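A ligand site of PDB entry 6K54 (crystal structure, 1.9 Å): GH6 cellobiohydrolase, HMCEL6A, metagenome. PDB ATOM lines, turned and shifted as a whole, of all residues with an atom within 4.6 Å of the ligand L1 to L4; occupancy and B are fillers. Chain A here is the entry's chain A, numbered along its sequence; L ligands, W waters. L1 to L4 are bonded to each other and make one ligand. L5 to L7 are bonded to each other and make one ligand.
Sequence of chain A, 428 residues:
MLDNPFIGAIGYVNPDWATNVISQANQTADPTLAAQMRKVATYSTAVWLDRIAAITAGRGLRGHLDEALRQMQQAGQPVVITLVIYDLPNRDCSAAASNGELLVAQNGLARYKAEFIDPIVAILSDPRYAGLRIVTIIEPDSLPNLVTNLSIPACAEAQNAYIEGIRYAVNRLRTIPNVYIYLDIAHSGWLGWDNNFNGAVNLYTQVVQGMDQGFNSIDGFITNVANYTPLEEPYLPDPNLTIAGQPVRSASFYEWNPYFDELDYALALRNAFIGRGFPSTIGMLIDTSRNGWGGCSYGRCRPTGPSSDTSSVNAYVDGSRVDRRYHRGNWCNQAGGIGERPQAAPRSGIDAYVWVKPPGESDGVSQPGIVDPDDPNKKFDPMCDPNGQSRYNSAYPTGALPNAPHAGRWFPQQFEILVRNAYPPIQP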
ATOM      1  N   TRP A  48      -4.832 -31.029  10.783  1.00  0.00           N
ATOM      2  CA  TRP A  48      -5.980 -30.148  10.926  1.00  0.00           C
ATOM      3  C   TRP A  48      -7.216 -30.750  10.264  1.00  0.00           C
ATOM      4  O   TRP A  48      -7.178 -31.135   9.101  1.00  0.00           O
ATOM      5  CB  TRP A  48      -5.685 -28.775  10.313  1.00  0.00           C
ATOM      6  CG  TRP A  48      -4.737 -27.935  11.137  1.00  0.00           C
ATOM      7  CD1 TRP A  48      -3.441 -28.233  11.456  1.00  0.00           C
ATOM      8  CD2 TRP A  48      -5.021 -26.681  11.753  1.00  0.00           C
ATOM      9  NE1 TRP A  48      -2.900 -27.225  12.232  1.00  0.00           N
ATOM     10  CE2 TRP A  48      -3.862 -26.267  12.434  1.00  0.00           C
ATOM     11  CE3 TRP A  48      -6.154 -25.860  11.788  1.00  0.00           C
ATOM     12  CZ2 TRP A  48      -3.795 -25.077  13.142  1.00  0.00           C
ATOM     13  CZ3 TRP A  48      -6.095 -24.681  12.496  1.00  0.00           C
ATOM     14  CH2 TRP A  48      -4.916 -24.289  13.166  1.00  0.00           C
ATOM     15  N   ASP A  50     -10.241 -29.311   9.082  1.00  0.00           N
ATOM     16  CA  ASP A  50     -10.635 -27.928   8.836  1.00  0.00           C
ATOM     17  C   ASP A  50     -11.888 -27.843   7.970  1.00  0.00           C
ATOM     18  O   ASP A  50     -12.291 -26.742   7.584  1.00  0.00           O
ATOM     19  CB  ASP A  50      -9.489 -27.147   8.197  1.00  0.00           C
ATOM     20  CG  ASP A  50      -9.078 -27.707   6.841  1.00  0.00           C
ATOM     21  OD1 ASP A  50      -9.200 -28.922   6.622  1.00  0.00           O
ATOM     22  OD2 ASP A  50      -8.624 -26.934   5.982  1.00  0.00           O
ATOM     23  N   ARG A  51     -12.515 -28.976   7.691  1.00  0.00           N
ATOM     24  CA  ARG A  51     -13.806 -29.008   7.004  1.00  0.00           C
ATOM     25  C   ARG A  51     -14.297 -30.447   7.024  1.00  0.00           C
ATOM     26  O   ARG A  51     -13.530 -31.376   7.281  1.00  0.00           O
ATOM     27  CB  ARG A  51     -13.729 -28.478   5.561  1.00  0.00           C
ATOM     28  CG  ARG A  51     -12.715 -29.145   4.653  1.00  0.00           C
ATOM     29  CD  ARG A  51     -12.661 -28.403   3.297  1.00  0.00           C
ATOM     30  NE  ARG A  51     -11.640 -28.982   2.433  1.00  0.00           N
ATOM     31  CZ  ARG A  51     -10.422 -28.476   2.238  1.00  0.00           C
ATOM     32  NH1 ARG A  51     -10.070 -27.342   2.839  1.00  0.00           N
ATOM     33  NH2 ARG A  51      -9.557 -29.087   1.444  1.00  0.00           N
ATOM     34  N   ALA A  57     -10.977 -37.008   3.115  1.00  0.00           N
ATOM     35  CA  ALA A  57     -10.170 -36.677   1.946  1.00  0.00           C
ATOM     36  C   ALA A  57      -8.776 -37.278   2.054  1.00  0.00           C
ATOM     37  O   ALA A  57      -8.152 -37.260   3.111  1.00  0.00           O
ATOM     38  CB  ALA A  57     -10.069 -35.163   1.782  1.00  0.00           C
ATOM     39  N   TYR A  86     -11.432 -27.978  13.845  1.00  0.00           N
ATOM     40  CA  TYR A  86     -11.430 -26.594  13.336  1.00  0.00           C
ATOM     41  C   TYR A  86     -12.526 -26.408  12.277  1.00  0.00           C
ATOM     42  O   TYR A  86     -12.247 -26.202  11.089  1.00  0.00           O
ATOM     43  CB  TYR A  86     -10.063 -26.242  12.774  1.00  0.00           C
ATOM     44  CG  TYR A  86      -9.868 -24.788  12.394  1.00  0.00           C
ATOM     45  CD1 TYR A  86     -10.074 -23.766  13.322  1.00  0.00           C
ATOM     46  CD2 TYR A  86      -9.467 -24.433  11.114  1.00  0.00           C
ATOM     47  CE1 TYR A  86      -9.882 -22.431  12.974  1.00  0.00           C
ATOM     48  CE2 TYR A  86      -9.284 -23.107  10.751  1.00  0.00           C
ATOM     49  CZ  TYR A  86      -9.482 -22.109  11.676  1.00  0.00           C
ATOM     50  OH  TYR A  86      -9.300 -20.784  11.314  1.00  0.00           O
ATOM     51  N   ARG A  91     -16.730 -19.586  11.584  1.00  0.00           N
ATOM     52  CA  ARG A  91     -15.327 -19.769  11.931  1.00  0.00           C
ATOM     53  C   ARG A  91     -14.515 -18.550  11.520  1.00  0.00           C
ATOM     54  O   ARG A  91     -14.840 -17.865  10.542  1.00  0.00           O
ATOM     55  CB  ARG A  91     -14.758 -21.020  11.250  1.00  0.00           C
ATOM     56  CG  ARG A  91     -13.389 -21.442  11.778  1.00  0.00           C
ATOM     57  CD  ARG A  91     -12.875 -22.644  11.014  1.00  0.00           C
ATOM     58  NE  ARG A  91     -12.384 -22.255   9.692  1.00  0.00           N
ATOM     59  CZ  ARG A  91     -12.112 -23.115   8.716  1.00  0.00           C
ATOM     60  NH1 ARG A  91     -11.672 -22.660   7.548  1.00  0.00           N
ATOM     61  NH2 ARG A  91     -12.264 -24.422   8.905  1.00  0.00           N
ATOM     62  N   ASP A  92     -13.451 -18.278  12.283  1.00  0.00           N
ATOM     63  CA  ASP A  92     -12.538 -17.174  12.000  1.00  0.00           C
ATOM     64  C   ASP A  92     -13.282 -15.847  12.000  1.00  0.00           C
ATOM     65  O   ASP A  92     -13.087 -14.999  11.119  1.00  0.00           O
ATOM     66  CB  ASP A  92     -11.797 -17.404  10.678  1.00  0.00           C
ATOM     67  CG  ASP A  92     -10.488 -16.610  10.579  1.00  0.00           C
ATOM     68  OD1 ASP A  92      -9.890 -16.291  11.647  1.00  0.00           O
ATOM     69  OD2 ASP A  92     -10.050 -16.326   9.439  1.00  0.00           O
ATOM     70  N   ALA A  97      -9.473 -14.595   6.137  1.00  0.00           N
ATOM     71  CA  ALA A  97      -8.636 -15.556   5.434  1.00  0.00           C
ATOM     72  C   ALA A  97      -9.084 -17.005   5.670  1.00  0.00           C
ATOM     73  O   ALA A  97      -8.875 -17.858   4.801  1.00  0.00           O
ATOM     74  CB  ALA A  97      -7.156 -15.391   5.842  1.00  0.00           C
ATOM     75  N   SER A  98      -9.710 -17.297   6.815  1.00  0.00           N
ATOM     76  CA  SER A  98     -10.036 -18.694   7.129  1.00  0.00           C
ATOM     77  C   SER A  98     -11.503 -18.895   7.509  1.00  0.00           C
ATOM     78  O   SER A  98     -11.833 -19.802   8.270  1.00  0.00           O
ATOM     79  CB  SER A  98      -9.133 -19.230   8.246  1.00  0.00           C
ATOM     80  OG  SER A  98      -7.811 -19.416   7.780  1.00  0.00           O
ATOM     81  N   PRO A 140      -9.160 -23.464  17.497  1.00  0.00           N
ATOM     82  CA  PRO A 140      -8.352 -22.237  17.602  1.00  0.00           C
ATOM     83  C   PRO A 140      -9.127 -20.974  17.249  1.00  0.00           C
ATOM     84  O   PRO A 140      -9.916 -20.959  16.306  1.00  0.00           O
ATOM     85  CB  PRO A 140      -7.212 -22.482  16.599  1.00  0.00           C
ATOM     86  CG  PRO A 140      -7.047 -23.977  16.602  1.00  0.00           C
ATOM     87  CD  PRO A 140      -8.441 -24.542  16.788  1.00  0.00           C
ATOM     88  N   ASP A 141      -8.885 -19.923  18.039  1.00  0.00           N
ATOM     89  CA  ASP A 141      -9.345 -18.537  17.822  1.00  0.00           C
ATOM     90  C   ASP A 141     -10.784 -18.288  18.278  1.00  0.00           C
ATOM     91  O   ASP A 141     -11.144 -17.128  18.550  1.00  0.00           O
ATOM     92  CB  ASP A 141      -9.226 -18.104  16.366  1.00  0.00           C
ATOM     93  CG  ASP A 141      -7.794 -18.201  15.833  1.00  0.00           C
ATOM     94  OD1 ASP A 141      -6.844 -18.126  16.646  1.00  0.00           O
ATOM     95  OD2 ASP A 141      -7.637 -18.374  14.592  1.00  0.00           O
ATOM     96  N   ALA A 226      -0.654 -21.188  15.434  1.00  0.00           N
ATOM     97  CA  ALA A 226      -0.493 -20.488  14.163  1.00  0.00           C
ATOM     98  C   ALA A 226       0.047 -19.077  14.328  1.00  0.00           C
ATOM     99  O   ALA A 226      -0.011 -18.294  13.367  1.00  0.00           O
ATOM    100  CB  ALA A 226      -1.820 -20.475  13.370  1.00  0.00           C
ATOM    101  N   ARG A 290       6.581 -21.620  14.544  1.00  0.00           N
ATOM    102  CA  ARG A 290       7.076 -20.482  13.759  1.00  0.00           C
ATOM    103  C   ARG A 290       7.484 -19.281  14.625  1.00  0.00           C
ATOM    104  O   ARG A 290       7.374 -18.130  14.176  1.00  0.00           O
ATOM    105  CB  ARG A 290       6.050 -20.035  12.704  1.00  0.00           C
ATOM    106  CG  ARG A 290       5.628 -21.155  11.719  1.00  0.00           C
ATOM    107  CD  ARG A 290       4.647 -20.652  10.636  1.00  0.00           C
ATOM    108  NE  ARG A 290       3.444 -20.070  11.213  1.00  0.00           N
ATOM    109  CZ  ARG A 290       2.432 -19.597  10.495  1.00  0.00           C
ATOM    110  NH1 ARG A 290       2.500 -19.647   9.169  1.00  0.00           N
ATOM    111  NH2 ARG A 290       1.372 -19.080  11.094  1.00  0.00           N
ATOM    112  N   TRP A 331      -0.477 -11.070  12.179  1.00  0.00           N
ATOM    113  CA  TRP A 331      -0.559 -12.518  12.269  1.00  0.00           C
ATOM    114  C   TRP A 331      -0.388 -13.239  10.939  1.00  0.00           C
ATOM    115  O   TRP A 331      -0.324 -14.467  10.927  1.00  0.00           O
ATOM    116  CB  TRP A 331      -1.892 -12.946  12.906  1.00  0.00           C
ATOM    117  CG  TRP A 331      -3.104 -12.346  12.228  1.00  0.00           C
ATOM    118  CD1 TRP A 331      -3.795 -11.236  12.616  1.00  0.00           C
ATOM    119  CD2 TRP A 331      -3.767 -12.841  11.051  1.00  0.00           C
ATOM    120  NE1 TRP A 331      -4.847 -10.998  11.744  1.00  0.00           N
ATOM    121  CE2 TRP A 331      -4.839 -11.959  10.778  1.00  0.00           C
ATOM    122  CE3 TRP A 331      -3.543 -13.927  10.200  1.00  0.00           C
ATOM    123  CZ2 TRP A 331      -5.701 -12.157   9.687  1.00  0.00           C
ATOM    124  CZ3 TRP A 331      -4.397 -14.113   9.109  1.00  0.00           C
ATOM    125  CH2 TRP A 331      -5.458 -13.223   8.865  1.00  0.00           C
ATOM    126  N   LYS A 357       0.332 -25.472  14.015  1.00  0.00           N
ATOM    127  CA  LYS A 357       0.422 -24.927  12.665  1.00  0.00           C
ATOM    128  C   LYS A 357       1.573 -25.598  11.920  1.00  0.00           C
ATOM    129  O   LYS A 357       2.705 -25.556  12.426  1.00  0.00           O
ATOM    130  CB  LYS A 357       0.666 -23.422  12.720  1.00  0.00           C
ATOM    131  CG  LYS A 357       0.967 -22.816  11.354  1.00  0.00           C
ATOM    132  CD  LYS A 357      -0.294 -22.829  10.479  1.00  0.00           C
ATOM    133  CE  LYS A 357      -0.088 -22.074   9.180  1.00  0.00           C
ATOM    134  NZ  LYS A 357      -1.327 -22.018   8.368  1.00  0.00           N
ATOM    135  N   PRO A 358       1.358 -26.230  10.768  1.00  0.00           N
ATOM    136  CA  PRO A 358       2.488 -26.897  10.104  1.00  0.00           C
ATOM    137  C   PRO A 358       3.319 -25.896   9.320  1.00  0.00           C
ATOM    138  O   PRO A 358       2.784 -25.174   8.468  1.00  0.00           O
ATOM    139  CB  PRO A 358       1.804 -27.915   9.179  1.00  0.00           C
ATOM    140  CG  PRO A 358       0.414 -28.062   9.719  1.00  0.00           C
ATOM    141  CD  PRO A 358       0.065 -26.675  10.212  1.00  0.00           C
ATOM    142  N   GLU A 361       2.675 -23.982   5.523  1.00  0.00           N
ATOM    143  CA  GLU A 361       1.296 -23.761   5.091  1.00  0.00           C
ATOM    144  C   GLU A 361       0.902 -22.294   5.289  1.00  0.00           C
ATOM    145  O   GLU A 361       1.233 -21.670   6.300  1.00  0.00           O
ATOM    146  CB  GLU A 361       0.361 -24.707   5.835  1.00  0.00           C
ATOM    147  CG  GLU A 361       0.629 -26.170   5.450  1.00  0.00           C
ATOM    148  CD  GLU A 361      -0.290 -27.185   6.136  1.00  0.00           C
ATOM    149  OE1 GLU A 361      -1.224 -26.766   6.861  1.00  0.00           O
ATOM    150  OE2 GLU A 361      -0.060 -28.411   5.943  1.00  0.00           O
ATOM    151  N   SER A 362       0.231 -21.748   4.277  1.00  0.00           N
ATOM    152  CA  SER A 362      -0.119 -20.322   4.253  1.00  0.00           C
ATOM    153  C   SER A 362      -1.131 -19.943   5.326  1.00  0.00           C
ATOM    154  O   SER A 362      -1.939 -20.772   5.774  1.00  0.00           O
ATOM    155  CB  SER A 362      -0.697 -19.978   2.876  1.00  0.00           C
ATOM    156  OG  SER A 362      -0.950 -18.599   2.750  1.00  0.00           O
ATOM    157  N   ASP A 363      -1.101 -18.661   5.739  1.00  0.00           N
ATOM    158  CA  ASP A 363      -2.128 -18.068   6.585  1.00  0.00           C
ATOM    159  C   ASP A 363      -3.231 -17.386   5.789  1.00  0.00           C
ATOM    160  O   ASP A 363      -4.228 -16.954   6.380  1.00  0.00           O
ATOM    161  CB  ASP A 363      -1.521 -17.033   7.563  1.00  0.00           C
ATOM    162  CG  ASP A 363      -0.390 -17.592   8.460  1.00  0.00           C
ATOM    163  OD1 ASP A 363      -0.475 -18.787   8.875  1.00  0.00           O
ATOM    164  OD2 ASP A 363       0.571 -16.817   8.762  1.00  0.00           O
ATOM    165  N   ASP A 375     -12.179 -24.355  -0.448  1.00  0.00           N
ATOM    166  CA  ASP A 375     -12.692 -23.582   0.681  1.00  0.00           C
ATOM    167  C   ASP A 375     -13.334 -22.345   0.076  1.00  0.00           C
ATOM    168  O   ASP A 375     -12.702 -21.283  -0.046  1.00  0.00           O
ATOM    169  CB  ASP A 375     -11.584 -23.174   1.653  1.00  0.00           C
ATOM    170  CG  ASP A 375     -10.966 -24.338   2.403  1.00  0.00           C
ATOM    171  OD1 ASP A 375     -11.717 -25.140   3.005  1.00  0.00           O
ATOM    172  OD2 ASP A 375      -9.708 -24.422   2.440  1.00  0.00           O
ATOM    173  N   LYS A 378     -13.062 -18.920   1.978  1.00  0.00           N
ATOM    174  CA  LYS A 378     -11.767 -18.289   2.230  1.00  0.00           C
ATOM    175  C   LYS A 378     -11.599 -17.079   1.315  1.00  0.00           C
ATOM    176  O   LYS A 378     -11.695 -17.198   0.092  1.00  0.00           O
ATOM    177  CB  LYS A 378     -10.639 -19.292   2.035  1.00  0.00           C
ATOM    178  CG  LYS A 378     -10.487 -20.198   3.245  1.00  0.00           C
ATOM    179  CD  LYS A 378      -9.330 -21.162   3.129  1.00  0.00           C
ATOM    180  CE  LYS A 378      -9.149 -21.927   4.443  1.00  0.00           C
ATOM    181  NZ  LYS A 378      -8.207 -23.087   4.288  1.00  0.00           N
ATOM    182  N   ALA A 407      -5.123 -19.786   2.629  1.00  0.00           N
ATOM    183  CA  ALA A 407      -4.720 -20.360   3.909  1.00  0.00           C
ATOM    184  C   ALA A 407      -4.697 -21.885   3.845  1.00  0.00           C
ATOM    185  O   ALA A 407      -5.622 -22.515   3.318  1.00  0.00           O
ATOM    186  CB  ALA A 407      -5.673 -19.903   5.012  1.00  0.00           C
ATOM    187  N   GLY A 408      -3.625 -22.472   4.367  1.00  0.00           N
ATOM    188  CA  GLY A 408      -3.448 -23.899   4.382  1.00  0.00           C
ATOM    189  C   GLY A 408      -2.738 -24.470   3.173  1.00  0.00           C
ATOM    190  O   GLY A 408      -2.228 -25.604   3.244  1.00  0.00           O
ATOM    191  N   ARG A 409      -2.679 -23.746   2.065  1.00  0.00           N
ATOM    192  CA  ARG A 409      -1.942 -24.277   0.921  1.00  0.00           C
ATOM    193  C   ARG A 409      -0.444 -24.024   1.086  1.00  0.00           C
ATOM    194  O   ARG A 409      -0.022 -23.130   1.828  1.00  0.00           O
ATOM    195  CB  ARG A 409      -2.456 -23.661  -0.387  1.00  0.00           C
ATOM    196  CG  ARG A 409      -3.909 -24.029  -0.682  1.00  0.00           C
ATOM    197  CD  ARG A 409      -4.205 -23.978  -2.175  1.00  0.00           C
ATOM    198  NE  ARG A 409      -5.593 -24.322  -2.475  1.00  0.00           N
ATOM    199  CZ  ARG A 409      -6.013 -25.534  -2.876  1.00  0.00           C
ATOM    200  NH1 ARG A 409      -5.147 -26.521  -3.020  1.00  0.00           N
ATOM    201  NH2 ARG A 409      -7.297 -25.735  -3.137  1.00  0.00           N
HETATM  202  C1  LIG L   1      -5.489 -17.655  10.290  1.00  0.00           C
HETATM  203  C2  LIG L   1      -4.138 -18.258  10.652  1.00  0.00           C
HETATM  204  C3  LIG L   1      -3.997 -19.370   9.636  1.00  0.00           C
HETATM  205  C4  LIG L   1      -5.006 -20.428  10.034  1.00  0.00           C
HETATM  206  C5  LIG L   1      -6.296 -19.918  10.749  1.00  0.00           C
HETATM  207  C6  LIG L   1      -6.478 -20.632  12.100  1.00  0.00           C
HETATM  208  O1  LIG L   1      -5.718 -17.662   8.849  1.00  0.00           O
HETATM  209  O2  LIG L   1      -3.079 -17.336  10.514  1.00  0.00           O
HETATM  210  O3  LIG L   1      -2.649 -19.884   9.557  1.00  0.00           O
HETATM  211  O4  LIG L   1      -5.336 -21.048   8.809  1.00  0.00           O
HETATM  212  O5  LIG L   1      -6.419 -18.508  10.977  1.00  0.00           O
HETATM  213  O6  LIG L   1      -5.355 -20.558  12.995  1.00  0.00           O
HETATM  214  C1  LG2 L   2      -6.246 -22.706   7.767  1.00  0.00           C
HETATM  215  C2  LG2 L   2      -6.425 -24.202   7.620  1.00  0.00           C
HETATM  216  C3  LG2 L   2      -5.062 -24.884   7.723  1.00  0.00           C
HETATM  217  C4  LG2 L   2      -4.361 -24.470   9.017  1.00  0.00           C
HETATM  218  C5  LG2 L   2      -2.953 -25.027   9.028  1.00  0.00           C
HETATM  219  C6  LG2 L   2      -5.522 -22.385   9.057  1.00  0.00           C
HETATM  220  O1  LG2 L   2      -7.511 -22.043   7.808  1.00  0.00           O
HETATM  221  O2  LG2 L   2      -7.016 -24.495   6.347  1.00  0.00           O
HETATM  222  O3  LG2 L   2      -5.230 -26.304   7.697  1.00  0.00           O
HETATM  223  O4  LG2 L   2      -4.261 -23.055   9.094  1.00  0.00           O
HETATM  224  O5  LG2 L   2      -2.298 -24.573   7.831  1.00  0.00           O
HETATM  225  C1  LG3 L   3      -4.277 -28.274   6.633  1.00  0.00           C
HETATM  226  C2  LG3 L   3      -3.838 -28.888   5.298  1.00  0.00           C
HETATM  227  C3  LG3 L   3      -4.849 -28.587   4.199  1.00  0.00           C
HETATM  228  C4  LG3 L   3      -5.126 -27.082   4.153  1.00  0.00           C
HETATM  229  C5  LG3 L   3      -6.128 -26.702   3.074  1.00  0.00           C
HETATM  230  C6  LG3 L   3      -4.748 -26.823   6.516  1.00  0.00           C
HETATM  231  O1  LG3 L   3      -3.194 -28.320   7.556  1.00  0.00           O
HETATM  232  O2  LG3 L   3      -3.729 -30.306   5.449  1.00  0.00           O
HETATM  233  O3  LG3 L   3      -4.285 -29.023   2.961  1.00  0.00           O
HETATM  234  O4  LG3 L   3      -5.652 -26.665   5.406  1.00  0.00           O
HETATM  235  O5  LG3 L   3      -7.346 -27.391   3.359  1.00  0.00           O
HETATM  236  C1  LG4 L   4      -4.482 -29.752   0.661  1.00  0.00           C
HETATM  237  C2  LG4 L   4      -5.276 -30.687  -0.238  1.00  0.00           C
HETATM  238  C3  LG4 L   4      -5.264 -32.099   0.324  1.00  0.00           C
HETATM  239  C4  LG4 L   4      -5.762 -32.082   1.765  1.00  0.00           C
HETATM  240  C5  LG4 L   4      -5.807 -33.482   2.370  1.00  0.00           C
HETATM  241  C6  LG4 L   4      -4.952 -29.875   2.114  1.00  0.00           C
HETATM  242  O1  LG4 L   4      -4.617 -28.387   0.215  1.00  0.00           O
HETATM  243  O2  LG4 L   4      -4.699 -30.692  -1.557  1.00  0.00           O
HETATM  244  O3  LG4 L   4      -6.120 -32.960  -0.447  1.00  0.00           O
HETATM  245  O4  LG4 L   4      -4.944 -31.230   2.567  1.00  0.00           O
HETATM  246  O5  LG4 L   4      -6.732 -33.464   3.463  1.00  0.00           O
HETATM  247  C1  LG5 L   5      -6.831  -6.394  21.080  1.00  0.00           C
HETATM  248  C2  LG5 L   5      -6.291  -7.788  20.730  1.00  0.00           C
HETATM  249  C3  LG5 L   5      -5.407  -7.723  19.493  1.00  0.00           C
HETATM  250  C4  LG5 L   5      -4.324  -6.677  19.643  1.00  0.00           C
HETATM  251  C5  LG5 L   5      -3.530  -6.515  18.353  1.00  0.00           C
HETATM  252  C6  LG5 L   5      -5.692  -5.395  21.170  1.00  0.00           C
HETATM  253  O1  LG5 L   5      -6.244  -4.094  21.397  1.00  0.00           O
HETATM  254  O2  LG5 L   5      -7.487  -6.385  22.351  1.00  0.00           O
HETATM  255  O3  LG5 L   5      -7.364  -8.700  20.463  1.00  0.00           O
HETATM  256  O4  LG5 L   5      -4.805  -9.007  19.276  1.00  0.00           O
HETATM  257  O5  LG5 L   5      -4.917  -5.410  19.978  1.00  0.00           O
HETATM  258  O6  LG5 L   5      -2.700  -5.380  18.453  1.00  0.00           O
HETATM  259  C1  LG6 L   6      -4.028 -10.782  17.978  1.00  0.00           C
HETATM  260  C2  LG6 L   6      -4.219 -11.521  16.677  1.00  0.00           C
HETATM  261  C3  LG6 L   6      -5.706 -11.822  16.413  1.00  0.00           C
HETATM  262  C4  LG6 L   6      -6.564 -10.558  16.577  1.00  0.00           C
HETATM  263  C5  LG6 L   6      -8.054 -10.843  16.443  1.00  0.00           C
HETATM  264  C6  LG6 L   6      -4.961  -9.566  18.031  1.00  0.00           C
HETATM  265  O1  LG6 L   6      -2.657 -10.345  18.096  1.00  0.00           O
HETATM  266  O2  LG6 L   6      -3.480 -12.735  16.767  1.00  0.00           O
HETATM  267  O3  LG6 L   6      -5.895 -12.262  15.076  1.00  0.00           O
HETATM  268  O4  LG6 L   6      -6.327  -9.961  17.852  1.00  0.00           O
HETATM  269  O5  LG6 L   6      -8.761  -9.586  16.512  1.00  0.00           O
HETATM  270  C1  LG7 L   7      -6.679 -13.814  13.495  1.00  0.00           C
HETATM  271  C2  LG7 L   7      -6.754 -15.300  13.202  1.00  0.00           C
HETATM  272  C3  LG7 L   7      -5.392 -15.942  13.431  1.00  0.00           C
HETATM  273  C4  LG7 L   7      -4.882 -15.623  14.836  1.00  0.00           C
HETATM  274  C5  LG7 L   7      -3.479 -16.189  15.068  1.00  0.00           C
HETATM  275  C6  LG7 L   7      -6.134 -13.604  14.900  1.00  0.00           C
HETATM  276  O1  LG7 L   7      -7.977 -13.236  13.396  1.00  0.00           O
HETATM  277  O2  LG7 L   7      -7.188 -15.433  11.850  1.00  0.00           O
HETATM  278  O3  LG7 L   7      -5.502 -17.366  13.326  1.00  0.00           O
HETATM  279  O4  LG7 L   7      -4.846 -14.217  15.004  1.00  0.00           O
HETATM  280  O5  LG7 L   7      -3.080 -15.946  16.421  1.00  0.00           O
HETATM  281  O   HOH W   1      -8.462 -33.202  -1.221  1.00  0.00           O
HETATM  282  O   HOH W   2      -1.147 -27.946   2.267  1.00  0.00           O
HETATM  283  O   HOH W   3      -5.660 -31.959   6.695  1.00  0.00           O
HETATM  284  O   HOH W   4      -4.862 -19.871  15.688  1.00  0.00           O
HETATM  285  O   HOH W   5      -7.996 -30.044   4.500  1.00  0.00           O
HETATM  286  O   HOH W   6      -7.554 -15.513   9.123  1.00  0.00           O
HETATM  287  O   HOH W   7      -2.146 -31.483  -1.705  1.00  0.00           O
HETATM  288  O   HOH W   8     -10.442 -24.574   5.882  1.00  0.00           O
HETATM  289  O   HOH W   9      -5.476 -34.740   6.014  1.00  0.00           O
HETATM  290  O   HOH W  10      -4.514 -33.746  -2.279  1.00  0.00           O
HETATM  291  O   HOH W  11      -2.148 -33.120   6.259  1.00  0.00           O
HETATM  292  O   HOH W  12      -7.669 -27.885  -0.105  1.00  0.00           O
HETATM  293  O   HOH W  13      -4.268 -36.037   0.709  1.00  0.00           O
HETATM  294  O   HOH W  14      -6.475 -29.613  -3.143  1.00  0.00           O
HETATM  295  O   HOH W  15      -3.060 -30.869   8.367  1.00  0.00           O
HETATM  296  O   HOH W  16      -7.903 -35.183   4.979  1.00  0.00           O
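An oxygen (O5) of LIG L1 is in hydrogen-bond range of an oxygen (O3) of LG7 L7.
OD1 of Asp 363 lies within salt-bridge range of NH2 of Arg 290, at 2.9 Å. OD2 of Asp 92 is in hydrogen-bond range of N of Ser 98, at 2.8 Å. The backbone carbonyl oxygen (O) of Ser 98 sits at hydrogen-bond distance from the guanidinium group (NE) of Arg 91, 2.9 Å away. NZ of Lys 378 is in hydrogen-bond range of O of Ala 407 (2.8 Å). The side-chain carboxylate (OD1) of Asp 375 lies within salt-bridge range of the guanidinium group (NH1) of Arg 51, at 2.8 Å. O of Tyr 86 sits at hydrogen-bond distance from NH2 of Arg 91 (2.8 Å). The guanidinium group (NH2) of Arg 91 lies within hydrogen-bond range of the backbone carbonyl oxygen (O) of Asp 50, 2.7 Å away. The backbone NH (N) of Ser 362 lies within hydrogen-bond range of the backbone carbonyl oxygen (O) of Arg 409 (2.8 Å).
Water W16 lies within hydrogen-bond range of an oxygen (O5) of LG4 L4 (2.6 Å) and the backbone carbonyl oxygen (O) of Ala 57 (2.8 Å). Water W14 lies within hydrogen-bond range of an oxygen (O2) of LG4 L4 and the guanidinium group of Arg 409. Water W3 lies within hydrogen-bond range of an oxygen (O2) of LG3 L3 (2.8 Å) and the backbone carbonyl oxygen (O) of Trp 48 (3.0 Å). Water W6 lies within hydrogen-bond range of OD2 of Asp 92, O2 of LG7 L7 and O1 of LIG L1. Water W12 bridges NH2 of Arg 51 (2.7 Å) and O1 of LG4 L4 (3.1 Å). Water W8 lies within hydrogen-bond range of the guanidinium group of Arg 91 (2.8 Å), the side-chain carboxylate of Asp 50 (3.0 Å), the side-chain amino group of Lys 378 (3.1 Å), the side-chain carboxylate of Asp 375 (3.2 Å) and an oxygen (O2) of LG2 L2 (3.5 Å).
An oxygen (O1) of LIG L1 is in hydrogen-bond range of the backbone carbonyl oxygen (O) of Asp 363, at 3.0 Å. The side-chain carboxylate of Asp 363 is in hydrogen-bond range of an oxygen (O3) of LIG L1, 2.5 Å away. OE1 of Glu 361 is in hydrogen-bond range of O1 of LG3 L3, at 2.6 Å. OG of Ser 98 lies within hydrogen-bond range of O1 of LG2 L2 (2.6 Å). The side-chain amino group (NZ) of Lys 378 is in hydrogen-bond range of an oxygen (O2) of LG2 L2 (2.8 Å). The guanidinium group (NH1) of Arg 51 lies within hydrogen-bond range of an oxygen (O5) of LG3 L3, at 2.8 Å. The side-chain amino group (NZ) of Lys 357 sits at hydrogen-bond distance from an oxygen (O3) of LIG L1, at 2.8 Å. OD2 of Asp 50 sits at hydrogen-bond distance from O2 of LG2 L2, at 2.9 Å. The side-chain carboxylate (OD2) of Asp 141 is in hydrogen-bond range of an oxygen (O3) of LG7 L7, at 2.7 Å. The side-chain carboxylate of Asp 92 is in hydrogen-bond range of an oxygen (O2) of LG7 L7.
CD2 of Trp 48 touches C4 of LG2 L2, at 3.6 Å. Tyr 86 touches the ligand L1 to L4. Asp 141 touches the ligand L1 to L4. Ala 226 touches the ligand L1 to L4. CE3 of Trp 331 touches O2 of LIG L1 (3.5 Å). Pro 358 touches the ligand L1 to L4. O of Ser 362 touches O3 of LIG L1, at 3.95 Å. OD2 of Asp 375 touches O5 of LG3 L3, at 3.9 Å. O of Ala 407 touches O2 of LG2 L2 (3.9 Å). O of Gly 408 touches C4 of LG3 L3, at 3.4 Å. NH1 of Arg 409 touches O1 of LG4 L4, at 3.8 Å. Hydrophobic or aromatic side chains that line the ligand L1 to L4: Trp 48, Tyr 86, Ala 226, Trp 331, Pro 358 and Ala 407. Of the 24 residues printed, 18 come within 4 Å of the ligand L1 to L4. The nearest printed residue that does not touch the ligand L1 to L4 is Ala 97 (4.03 Å).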
